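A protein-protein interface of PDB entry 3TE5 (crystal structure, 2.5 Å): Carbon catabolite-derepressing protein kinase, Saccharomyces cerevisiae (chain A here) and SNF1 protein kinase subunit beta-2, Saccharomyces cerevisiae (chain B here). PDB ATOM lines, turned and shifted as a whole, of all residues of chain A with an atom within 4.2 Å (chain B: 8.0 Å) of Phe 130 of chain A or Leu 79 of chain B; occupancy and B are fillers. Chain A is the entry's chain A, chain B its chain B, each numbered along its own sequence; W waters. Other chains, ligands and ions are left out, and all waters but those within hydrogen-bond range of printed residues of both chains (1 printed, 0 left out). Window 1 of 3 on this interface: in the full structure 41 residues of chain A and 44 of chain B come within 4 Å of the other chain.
The backbone NH of Leu 79 of chain B lies within hydrogen-bond range of the backbone carbonyl oxygen of Phe 130 of chain A (2.9 Å). N of Gly 54 of chain A lies within hydrogen-bond range of O of Leu 79 of chain B, at 2.9 Å. A ring nitrogen (ND1) of His 78 of chain B is in hydrogen-bond range of the side-chain carboxylate (OD1) of Asp 129 of chain A. OG1 of Thr 81 of chain B is in hydrogen-bond range of O of Gly 54 of chain A (2.7 Å).
The backbone carbonyl oxygen (O) of Ala 92 of chain B lies within hydrogen-bond range of the backbone NH (N) of Val 80 of chain B (2.6 Å). N of Val 115 of chain A sits at hydrogen-bond distance from O of Lys 131 of chain A (2.8 Å). N of Asn 77 of chain B sits at hydrogen-bond distance from O of Ile 94 of chain B (2.8 Å). The side-chain hydroxyl of Thr 165 of chain A is in hydrogen-bond range of the backbone carbonyl oxygen of Leu 162 of chain A (2.9 Å). The backbone carbonyl oxygen of Ser 93 of chain B is in hydrogen-bond range of the backbone NH of Gln 104 of chain B, 2.9 Å away. The backbone carbonyl oxygen of Phe 161 of chain A lies close to the side-chain hydroxyl of Thr 165 of chain A, 3.4 Å away.
Phe 53 of chain A touches Leu 45 of chain B (CD2 to O, 3.4 Å). CZ of Phe 53 of chain A touches CB of Val 75 of chain B (3.4 Å). Phe 53 of chain A touches Leu 79 of chain B (CA to O, 3.4 Å). Asn 77 of chain B touches Phe 130 of chain A. CA of His 78 of chain B touches O of Phe 130 of chain A, at 3.3 Å. Lys 131 of chain A touches His 78 of chain B (CE to NE2, 3.4 Å). CD2 of Leu 162 of chain A touches CD1 of Leu 79 of chain B (3.8 Å). Val 91 of chain B touches Leu 162 of chain A (CG2 to O, 3.8 Å). CD2 of Leu 162 of chain A touches N of Ser 93 of chain B, at 3.8 Å. Ile 169 of chain A touches Leu 79 of chain B (CD1 to CD2, 3.8 Å).
Asp 129 of chain A touches one residue of chain B. Printed residues of chain A within 4 Å of Leu 50 of chain B: Phe 53. Of the printed residues of chain A, Val 75 of chain B touches Phe 53. Of the printed residues of chain A, His 78 of chain B touches Asp 129, Phe 130 and Lys 131. Of chain A, only Phe 53 (3.4 Å), Gly 54 (2.9 Å), Phe 130 (2.9 Å), Leu 162 (3.8 Å), Thr 165 (3.4 Å) and Ile 169 (3.8 Å) come within 4 Å of Leu 79 of chain B. Of the printed residues of chain A, Val 80 of chain B touches Phe 53 (3.8 Å). Ile 94 of chain B touches none of the printed residues of chain A. Of the printed residues of chain A, Gln 104 of chain B touches Leu 162 (3.4 Å). The nearest printed residue of chain B that does not touch Phe 130 of chain A is Val 80 of chain B (6.2 Å). The nearest residue of chain A that does not touch Leu 79 of chain B is Phe 161 of chain A (4.1 Å). The nearest printed residue of chain A that does not touch Leu 45 of chain B is Asp 129 of chain A (4.3 Å).
Of the 17 printed residues of chain B, 13 touch a printed residue of chain A. Hydrophobic or aromatic side chains of chain B within 4 Å of the printed part of chain A: Leu 45, Leu 50, Val 75, His 78, Leu 79, Val 80 and Val 91.
Water W1 lies within hydrogen-bond range of OD1 of Asp 129 of chain A, O of Leu 79 of chain B, N of Phe 130 of chain A and N of Gly 54 of chain A.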
ATOM      1  N   PHE A  53      -9.694 -27.622  12.167  1.00  0.00           N
ATOM      2  CA  PHE A  53      -8.732 -26.619  12.596  1.00  0.00           C
ATOM      3  C   PHE A  53      -9.479 -25.520  13.333  1.00  0.00           C
ATOM      4  O   PHE A  53     -10.512 -25.048  12.864  1.00  0.00           O
ATOM      5  CB  PHE A  53      -7.955 -26.046  11.411  1.00  0.00           C
ATOM      6  CG  PHE A  53      -6.948 -26.990  10.844  1.00  0.00           C
ATOM      7  CD1 PHE A  53      -5.764 -27.261  11.530  1.00  0.00           C
ATOM      8  CD2 PHE A  53      -7.180 -27.621   9.626  1.00  0.00           C
ATOM      9  CE1 PHE A  53      -4.827 -28.145  11.007  1.00  0.00           C
ATOM     10  CE2 PHE A  53      -6.246 -28.505   9.096  1.00  0.00           C
ATOM     11  CZ  PHE A  53      -5.072 -28.768   9.788  1.00  0.00           C
ATOM     12  N   GLY A  54      -8.964 -25.150  14.502  1.00  0.00           N
ATOM     13  CA  GLY A  54      -9.561 -24.125  15.352  1.00  0.00           C
ATOM     14  C   GLY A  54     -11.030 -24.324  15.684  1.00  0.00           C
ATOM     15  O   GLY A  54     -11.546 -25.443  15.657  1.00  0.00           O
ATOM     16  N   ILE A  55     -11.702 -23.220  15.998  1.00  0.00           N
ATOM     17  CA  ILE A  55     -13.129 -23.233  16.314  1.00  0.00           C
ATOM     18  C   ILE A  55     -13.921 -22.380  15.329  1.00  0.00           C
ATOM     19  O   ILE A  55     -13.423 -21.373  14.821  1.00  0.00           O
ATOM     20  CB  ILE A  55     -13.411 -22.783  17.771  1.00  0.00           C
ATOM     21  CG1 ILE A  55     -12.695 -21.465  18.089  1.00  0.00           C
ATOM     22  CG2 ILE A  55     -13.001 -23.888  18.755  1.00  0.00           C
ATOM     23  CD1 ILE A  55     -13.209 -20.759  19.333  1.00  0.00           C
ATOM     24  N   MET A 114       1.556 -16.414  20.232  1.00  0.00           N
ATOM     25  CA  MET A 114       0.505 -17.022  19.430  1.00  0.00           C
ATOM     26  C   MET A 114       0.064 -16.068  18.338  1.00  0.00           C
ATOM     27  O   MET A 114       0.083 -14.850  18.521  1.00  0.00           O
ATOM     28  CB  MET A 114      -0.703 -17.366  20.295  1.00  0.00           C
ATOM     29  CG  MET A 114      -0.588 -18.642  21.091  1.00  0.00           C
ATOM     30  SD  MET A 114      -2.060 -18.937  22.089  1.00  0.00           S
ATOM     31  CE  MET A 114      -3.338 -18.975  20.834  1.00  0.00           C
ATOM     32  N   VAL A 115      -0.329 -16.625  17.200  1.00  0.00           N
ATOM     33  CA  VAL A 115      -0.948 -15.839  16.148  1.00  0.00           C
ATOM     34  C   VAL A 115      -2.352 -16.380  15.904  1.00  0.00           C
ATOM     35  O   VAL A 115      -2.522 -17.520  15.467  1.00  0.00           O
ATOM     36  CB  VAL A 115      -0.109 -15.828  14.845  1.00  0.00           C
ATOM     37  CG1 VAL A 115      -0.870 -15.148  13.711  1.00  0.00           C
ATOM     38  CG2 VAL A 115       1.227 -15.134  15.076  1.00  0.00           C
ATOM     39  N   ILE A 116      -3.354 -15.561  16.221  1.00  0.00           N
ATOM     40  CA  ILE A 116      -4.744 -15.912  15.959  1.00  0.00           C
ATOM     41  C   ILE A 116      -5.212 -15.218  14.685  1.00  0.00           C
ATOM     42  O   ILE A 116      -4.966 -14.028  14.491  1.00  0.00           O
ATOM     43  CB  ILE A 116      -5.671 -15.570  17.155  1.00  0.00           C
ATOM     44  CG1 ILE A 116      -5.276 -16.396  18.386  1.00  0.00           C
ATOM     45  CG2 ILE A 116      -7.139 -15.813  16.789  1.00  0.00           C
ATOM     46  CD1 ILE A 116      -6.076 -16.087  19.643  1.00  0.00           C
ATOM     47  N   VAL A 128     -11.897 -19.477  13.564  1.00  0.00           N
ATOM     48  CA  VAL A 128     -10.851 -18.874  14.375  1.00  0.00           C
ATOM     49  C   VAL A 128      -9.654 -19.822  14.407  1.00  0.00           C
ATOM     50  O   VAL A 128      -9.705 -20.886  15.035  1.00  0.00           O
ATOM     51  CB  VAL A 128     -11.334 -18.573  15.810  1.00  0.00           C
ATOM     52  CG1 VAL A 128     -10.300 -17.747  16.548  1.00  0.00           C
ATOM     53  CG2 VAL A 128     -12.673 -17.845  15.789  1.00  0.00           C
ATOM     54  N   ASP A 129      -8.590 -19.428  13.713  1.00  0.00           N
ATOM     55  CA  ASP A 129      -7.384 -20.236  13.587  1.00  0.00           C
ATOM     56  C   ASP A 129      -6.340 -19.823  14.618  1.00  0.00           C
ATOM     57  O   ASP A 129      -6.027 -18.644  14.760  1.00  0.00           O
ATOM     58  CB  ASP A 129      -6.816 -20.123  12.168  1.00  0.00           C
ATOM     59  CG  ASP A 129      -5.452 -20.779  12.022  1.00  0.00           C
ATOM     60  OD1 ASP A 129      -5.346 -22.012  12.214  1.00  0.00           O
ATOM     61  OD2 ASP A 129      -4.484 -20.056  11.703  1.00  0.00           O
ATOM     62  N   PHE A 130      -5.807 -20.812  15.328  1.00  0.00           N
ATOM     63  CA  PHE A 130      -4.804 -20.584  16.360  1.00  0.00           C
ATOM     64  C   PHE A 130      -3.476 -21.186  15.920  1.00  0.00           C
ATOM     65  O   PHE A 130      -3.421 -22.340  15.493  1.00  0.00           O
ATOM     66  CB  PHE A 130      -5.234 -21.217  17.687  1.00  0.00           C
ATOM     67  CG  PHE A 130      -6.564 -20.732  18.202  1.00  0.00           C
ATOM     68  CD1 PHE A 130      -6.626 -19.734  19.169  1.00  0.00           C
ATOM     69  CD2 PHE A 130      -7.752 -21.293  17.742  1.00  0.00           C
ATOM     70  CE1 PHE A 130      -7.852 -19.291  19.657  1.00  0.00           C
ATOM     71  CE2 PHE A 130      -8.976 -20.857  18.223  1.00  0.00           C
ATOM     72  CZ  PHE A 130      -9.028 -19.854  19.181  1.00  0.00           C
ATOM     73  N   LYS A 131      -2.410 -20.405  16.033  1.00  0.00           N
ATOM     74  CA  LYS A 131      -1.089 -20.851  15.617  1.00  0.00           C
ATOM     75  C   LYS A 131      -0.049 -20.557  16.691  1.00  0.00           C
ATOM     76  O   LYS A 131       0.061 -19.428  17.168  1.00  0.00           O
ATOM     77  CB  LYS A 131      -0.698 -20.176  14.302  1.00  0.00           C
ATOM     78  CG  LYS A 131       0.415 -20.864  13.532  1.00  0.00           C
ATOM     79  CD  LYS A 131       0.912 -19.970  12.399  1.00  0.00           C
ATOM     80  CE  LYS A 131       1.811 -20.721  11.421  1.00  0.00           C
ATOM     81  NZ  LYS A 131       3.049 -21.250  12.060  1.00  0.00           N
ATOM     82  N   PHE A 161       1.186 -24.897  24.576  1.00  0.00           N
ATOM     83  CA  PHE A 161       0.328 -24.203  23.626  1.00  0.00           C
ATOM     84  C   PHE A 161      -1.078 -24.792  23.647  1.00  0.00           C
ATOM     85  O   PHE A 161      -2.058 -24.052  23.712  1.00  0.00           O
ATOM     86  CB  PHE A 161       0.947 -24.263  22.220  1.00  0.00           C
ATOM     87  CG  PHE A 161      -0.018 -23.967  21.102  1.00  0.00           C
ATOM     88  CD1 PHE A 161      -0.421 -22.660  20.834  1.00  0.00           C
ATOM     89  CD2 PHE A 161      -0.507 -24.995  20.301  1.00  0.00           C
ATOM     90  CE1 PHE A 161      -1.304 -22.390  19.795  1.00  0.00           C
ATOM     91  CE2 PHE A 161      -1.394 -24.734  19.262  1.00  0.00           C
ATOM     92  CZ  PHE A 161      -1.794 -23.427  19.009  1.00  0.00           C
ATOM     93  N   LEU A 162      -1.165 -26.120  23.617  1.00  0.00           N
ATOM     94  CA  LEU A 162      -2.449 -26.823  23.613  1.00  0.00           C
ATOM     95  C   LEU A 162      -3.250 -26.570  24.888  1.00  0.00           C
ATOM     96  O   LEU A 162      -4.473 -26.422  24.844  1.00  0.00           O
ATOM     97  CB  LEU A 162      -2.242 -28.331  23.410  1.00  0.00           C
ATOM     98  CG  LEU A 162      -1.700 -28.813  22.059  1.00  0.00           C
ATOM     99  CD1 LEU A 162      -1.454 -30.323  22.077  1.00  0.00           C
ATOM    100  CD2 LEU A 162      -2.615 -28.426  20.904  1.00  0.00           C
ATOM    101  N   THR A 165      -4.567 -22.851  24.772  1.00  0.00           N
ATOM    102  CA  THR A 165      -5.705 -22.713  23.864  1.00  0.00           C
ATOM    103  C   THR A 165      -6.951 -23.309  24.511  1.00  0.00           C
ATOM    104  O   THR A 165      -8.053 -22.793  24.342  1.00  0.00           O
ATOM    105  CB  THR A 165      -5.458 -23.339  22.470  1.00  0.00           C
ATOM    106  OG1 THR A 165      -5.191 -24.739  22.595  1.00  0.00           O
ATOM    107  CG2 THR A 165      -4.290 -22.657  21.773  1.00  0.00           C
ATOM    108  N   LEU A 168      -8.302 -20.746  26.662  1.00  0.00           N
ATOM    109  CA  LEU A 168      -8.893 -19.748  25.783  1.00  0.00           C
ATOM    110  C   LEU A 168     -10.240 -20.195  25.222  1.00  0.00           C
ATOM    111  O   LEU A 168     -11.210 -19.438  25.281  1.00  0.00           O
ATOM    112  CB  LEU A 168      -7.915 -19.403  24.655  1.00  0.00           C
ATOM    113  CG  LEU A 168      -8.170 -18.190  23.754  1.00  0.00           C
ATOM    114  CD1 LEU A 168      -8.559 -16.953  24.553  1.00  0.00           C
ATOM    115  CD2 LEU A 168      -6.933 -17.915  22.921  1.00  0.00           C
ATOM    116  N   ILE A 169     -10.298 -21.418  24.696  1.00  0.00           N
ATOM    117  CA  ILE A 169     -11.538 -21.989  24.157  1.00  0.00           C
ATOM    118  C   ILE A 169     -12.642 -22.021  25.218  1.00  0.00           C
ATOM    119  O   ILE A 169     -13.803 -21.722  24.926  1.00  0.00           O
ATOM    120  CB  ILE A 169     -11.322 -23.423  23.590  1.00  0.00           C
ATOM    121  CG1 ILE A 169     -10.347 -23.406  22.404  1.00  0.00           C
ATOM    122  CG2 ILE A 169     -12.653 -24.059  23.168  1.00  0.00           C
ATOM    123  CD1 ILE A 169      -9.674 -24.749  22.138  1.00  0.00           C
ATOM    124  N   LEU B  45      -6.489 -25.680   5.109  1.00  0.00           N
ATOM    125  CA  LEU B  45      -7.129 -25.720   6.422  1.00  0.00           C
ATOM    126  C   LEU B  45      -8.568 -26.242   6.380  1.00  0.00           C
ATOM    127  O   LEU B  45      -9.294 -26.141   7.368  1.00  0.00           O
ATOM    128  CB  LEU B  45      -7.077 -24.342   7.098  1.00  0.00           C
ATOM    129  CG  LEU B  45      -5.708 -23.766   7.486  1.00  0.00           C
ATOM    130  CD1 LEU B  45      -5.855 -22.317   7.922  1.00  0.00           C
ATOM    131  CD2 LEU B  45      -5.025 -24.585   8.579  1.00  0.00           C
ATOM    132  N   LEU B  50      -8.183 -32.290   6.231  1.00  0.00           N
ATOM    133  CA  LEU B  50      -7.639 -32.671   7.540  1.00  0.00           C
ATOM    134  C   LEU B  50      -8.029 -34.092   7.967  1.00  0.00           C
ATOM    135  O   LEU B  50      -7.217 -34.806   8.557  1.00  0.00           O
ATOM    136  CB  LEU B  50      -8.054 -31.657   8.613  1.00  0.00           C
ATOM    137  CG  LEU B  50      -7.845 -31.975  10.100  1.00  0.00           C
ATOM    138  CD1 LEU B  50      -6.374 -32.151  10.462  1.00  0.00           C
ATOM    139  CD2 LEU B  50      -8.466 -30.892  10.958  1.00  0.00           C
ATOM    140  N   VAL B  75      -0.253 -26.372   7.608  1.00  0.00           N
ATOM    141  CA  VAL B  75      -1.047 -26.692   8.799  1.00  0.00           C
ATOM    142  C   VAL B  75      -0.219 -26.918  10.067  1.00  0.00           C
ATOM    143  O   VAL B  75      -0.777 -27.057  11.159  1.00  0.00           O
ATOM    144  CB  VAL B  75      -1.991 -27.901   8.565  1.00  0.00           C
ATOM    145  CG1 VAL B  75      -2.804 -27.711   7.284  1.00  0.00           C
ATOM    146  CG2 VAL B  75      -1.219 -29.216   8.535  1.00  0.00           C
ATOM    147  N   LEU B  76       1.102 -26.946   9.921  1.00  0.00           N
ATOM    148  CA  LEU B  76       1.989 -27.182  11.056  1.00  0.00           C
ATOM    149  C   LEU B  76       1.835 -26.119  12.138  1.00  0.00           C
ATOM    150  O   LEU B  76       1.743 -24.932  11.840  1.00  0.00           O
ATOM    151  CB  LEU B  76       3.448 -27.294  10.603  1.00  0.00           C
ATOM    152  CG  LEU B  76       3.835 -28.575   9.851  1.00  0.00           C
ATOM    153  CD1 LEU B  76       5.194 -28.420   9.182  1.00  0.00           C
ATOM    154  CD2 LEU B  76       3.816 -29.790  10.771  1.00  0.00           C
ATOM    155  N   ASN B  77       1.791 -26.572  13.392  1.00  0.00           N
ATOM    156  CA  ASN B  77       1.644 -25.705  14.574  1.00  0.00           C
ATOM    157  C   ASN B  77       0.301 -24.967  14.679  1.00  0.00           C
ATOM    158  O   ASN B  77       0.173 -24.013  15.444  1.00  0.00           O
ATOM    159  CB  ASN B  77       2.827 -24.733  14.708  1.00  0.00           C
ATOM    160  CG  ASN B  77       4.174 -25.429  14.586  1.00  0.00           C
ATOM    161  OD1 ASN B  77       4.404 -26.475  15.192  1.00  0.00           O
ATOM    162  ND2 ASN B  77       5.069 -24.852  13.790  1.00  0.00           N
ATOM    163  N   HIS B  78      -0.692 -25.423  13.917  1.00  0.00           N
ATOM    164  CA  HIS B  78      -2.057 -24.914  14.027  1.00  0.00           C
ATOM    165  C   HIS B  78      -2.909 -25.820  14.914  1.00  0.00           C
ATOM    166  O   HIS B  78      -2.819 -27.051  14.831  1.00  0.00           O
ATOM    167  CB  HIS B  78      -2.708 -24.785  12.650  1.00  0.00           C
ATOM    168  CG  HIS B  78      -2.108 -23.713  11.793  1.00  0.00           C
ATOM    169  ND1 HIS B  78      -2.639 -22.444  11.709  1.00  0.00           N
ATOM    170  CD2 HIS B  78      -1.026 -23.724  10.980  1.00  0.00           C
ATOM    171  CE1 HIS B  78      -1.907 -21.719  10.882  1.00  0.00           C
ATOM    172  NE2 HIS B  78      -0.923 -22.472  10.427  1.00  0.00           N
ATOM    173  N   LEU B  79      -3.742 -25.204  15.749  1.00  0.00           N
ATOM    174  CA  LEU B  79      -4.628 -25.933  16.652  1.00  0.00           C
ATOM    175  C   LEU B  79      -5.673 -26.770  15.913  1.00  0.00           C
ATOM    176  O   LEU B  79      -6.336 -26.289  14.989  1.00  0.00           O
ATOM    177  CB  LEU B  79      -5.321 -24.973  17.629  1.00  0.00           C
ATOM    178  CG  LEU B  79      -6.293 -25.596  18.641  1.00  0.00           C
ATOM    179  CD1 LEU B  79      -5.547 -26.439  19.654  1.00  0.00           C
ATOM    180  CD2 LEU B  79      -7.115 -24.534  19.340  1.00  0.00           C
ATOM    181  N   VAL B  80      -5.799 -28.027  16.328  1.00  0.00           N
ATOM    182  CA  VAL B  80      -6.869 -28.902  15.865  1.00  0.00           C
ATOM    183  C   VAL B  80      -7.806 -29.159  17.043  1.00  0.00           C
ATOM    184  O   VAL B  80      -7.356 -29.324  18.176  1.00  0.00           O
ATOM    185  CB  VAL B  80      -6.326 -30.251  15.325  1.00  0.00           C
ATOM    186  CG1 VAL B  80      -7.436 -31.055  14.669  1.00  0.00           C
ATOM    187  CG2 VAL B  80      -5.191 -30.025  14.334  1.00  0.00           C
ATOM    188  N   THR B  81      -9.107 -29.168  16.778  1.00  0.00           N
ATOM    189  CA  THR B  81     -10.095 -29.423  17.819  1.00  0.00           C
ATOM    190  C   THR B  81     -11.090 -30.475  17.373  1.00  0.00           C
ATOM    191  O   THR B  81     -11.086 -30.912  16.221  1.00  0.00           O
ATOM    192  CB  THR B  81     -10.889 -28.145  18.218  1.00  0.00           C
ATOM    193  OG1 THR B  81     -11.660 -27.688  17.102  1.00  0.00           O
ATOM    194  CG2 THR B  81      -9.966 -27.032  18.688  1.00  0.00           C
ATOM    195  N   SER B  82     -11.935 -30.878  18.312  1.00  0.00           N
ATOM    196  CA  SER B  82     -13.071 -31.743  18.049  1.00  0.00           C
ATOM    197  C   SER B  82     -14.159 -31.359  19.044  1.00  0.00           C
ATOM    198  O   SER B  82     -13.934 -30.500  19.897  1.00  0.00           O
ATOM    199  CB  SER B  82     -12.672 -33.213  18.199  1.00  0.00           C
ATOM    200  OG  SER B  82     -11.940 -33.429  19.395  1.00  0.00           O
ATOM    201  N   LEU B  89     -11.968 -32.050  26.884  1.00  0.00           N
ATOM    202  CA  LEU B  89     -11.518 -31.353  25.692  1.00  0.00           C
ATOM    203  C   LEU B  89     -10.424 -32.171  25.014  1.00  0.00           C
ATOM    204  O   LEU B  89      -9.569 -32.766  25.677  1.00  0.00           O
ATOM    205  CB  LEU B  89     -11.008 -29.962  26.061  1.00  0.00           C
ATOM    206  CG  LEU B  89     -10.951 -28.873  24.987  1.00  0.00           C
ATOM    207  CD1 LEU B  89     -12.231 -28.790  24.152  1.00  0.00           C
ATOM    208  CD2 LEU B  89     -10.662 -27.541  25.647  1.00  0.00           C
ATOM    209  N   CYS B  90     -10.477 -32.218  23.690  1.00  0.00           N
ATOM    210  CA  CYS B  90      -9.486 -32.931  22.914  1.00  0.00           C
ATOM    211  C   CYS B  90      -8.942 -32.028  21.827  1.00  0.00           C
ATOM    212  O   CYS B  90      -9.582 -31.823  20.795  1.00  0.00           O
ATOM    213  CB  CYS B  90     -10.075 -34.202  22.307  1.00  0.00           C
ATOM    214  SG  CYS B  90      -8.843 -35.211  21.446  1.00  0.00           S
ATOM    215  N   VAL B  91      -7.757 -31.485  22.077  1.00  0.00           N
ATOM    216  CA  VAL B  91      -7.077 -30.628  21.119  1.00  0.00           C
ATOM    217  C   VAL B  91      -5.813 -31.294  20.594  1.00  0.00           C
ATOM    218  O   VAL B  91      -5.288 -32.229  21.207  1.00  0.00           O
ATOM    219  CB  VAL B  91      -6.731 -29.249  21.716  1.00  0.00           C
ATOM    220  CG1 VAL B  91      -8.002 -28.427  21.944  1.00  0.00           C
ATOM    221  CG2 VAL B  91      -5.912 -29.391  23.001  1.00  0.00           C
ATOM    222  N   ALA B  92      -5.328 -30.806  19.455  1.00  0.00           N
ATOM    223  CA  ALA B  92      -4.144 -31.371  18.821  1.00  0.00           C
ATOM    224  C   ALA B  92      -3.388 -30.330  18.020  1.00  0.00           C
ATOM    225  O   ALA B  92      -3.943 -29.300  17.630  1.00  0.00           O
ATOM    226  CB  ALA B  92      -4.522 -32.550  17.934  1.00  0.00           C
ATOM    227  N   SER B  93      -2.108 -30.600  17.792  1.00  0.00           N
ATOM    228  CA  SER B  93      -1.323 -29.819  16.851  1.00  0.00           C
ATOM    229  C   SER B  93      -0.351 -30.718  16.100  1.00  0.00           C
ATOM    230  O   SER B  93       0.377 -31.511  16.704  1.00  0.00           O
ATOM    231  CB  SER B  93      -0.577 -28.692  17.561  1.00  0.00           C
ATOM    232  OG  SER B  93       0.096 -27.880  16.617  1.00  0.00           O
ATOM    233  N   ILE B  94      -0.366 -30.602  14.777  1.00  0.00           N
ATOM    234  CA  ILE B  94       0.579 -31.312  13.930  1.00  0.00           C
ATOM    235  C   ILE B  94       1.889 -30.539  13.952  1.00  0.00           C
ATOM    236  O   ILE B  94       1.949 -29.385  13.528  1.00  0.00           O
ATOM    237  CB  ILE B  94       0.062 -31.446  12.482  1.00  0.00           C
ATOM    238  CG1 ILE B  94      -1.378 -31.976  12.482  1.00  0.00           C
ATOM    239  CG2 ILE B  94       0.999 -32.341  11.657  1.00  0.00           C
ATOM    240  CD1 ILE B  94      -2.079 -31.882  11.144  1.00  0.00           C
ATOM    241  N   GLN B 104       0.416 -34.152  17.881  1.00  0.00           N
ATOM    242  CA  GLN B 104       0.399 -34.152  19.340  1.00  0.00           C
ATOM    243  C   GLN B 104      -1.007 -33.873  19.875  1.00  0.00           C
ATOM    244  O   GLN B 104      -1.536 -32.774  19.727  1.00  0.00           O
ATOM    245  CB  GLN B 104       1.423 -33.159  19.898  1.00  0.00           C
ATOM    246  CG  GLN B 104       2.862 -33.533  19.562  1.00  0.00           C
ATOM    247  CD  GLN B 104       3.885 -32.520  20.035  1.00  0.00           C
ATOM    248  OE1 GLN B 104       3.548 -31.502  20.637  1.00  0.00           O
ATOM    249  NE2 GLN B 104       5.147 -32.798  19.764  1.00  0.00           N
HETATM  250  O   HOH W   1      -6.246 -23.516  14.404  1.00  0.00           O
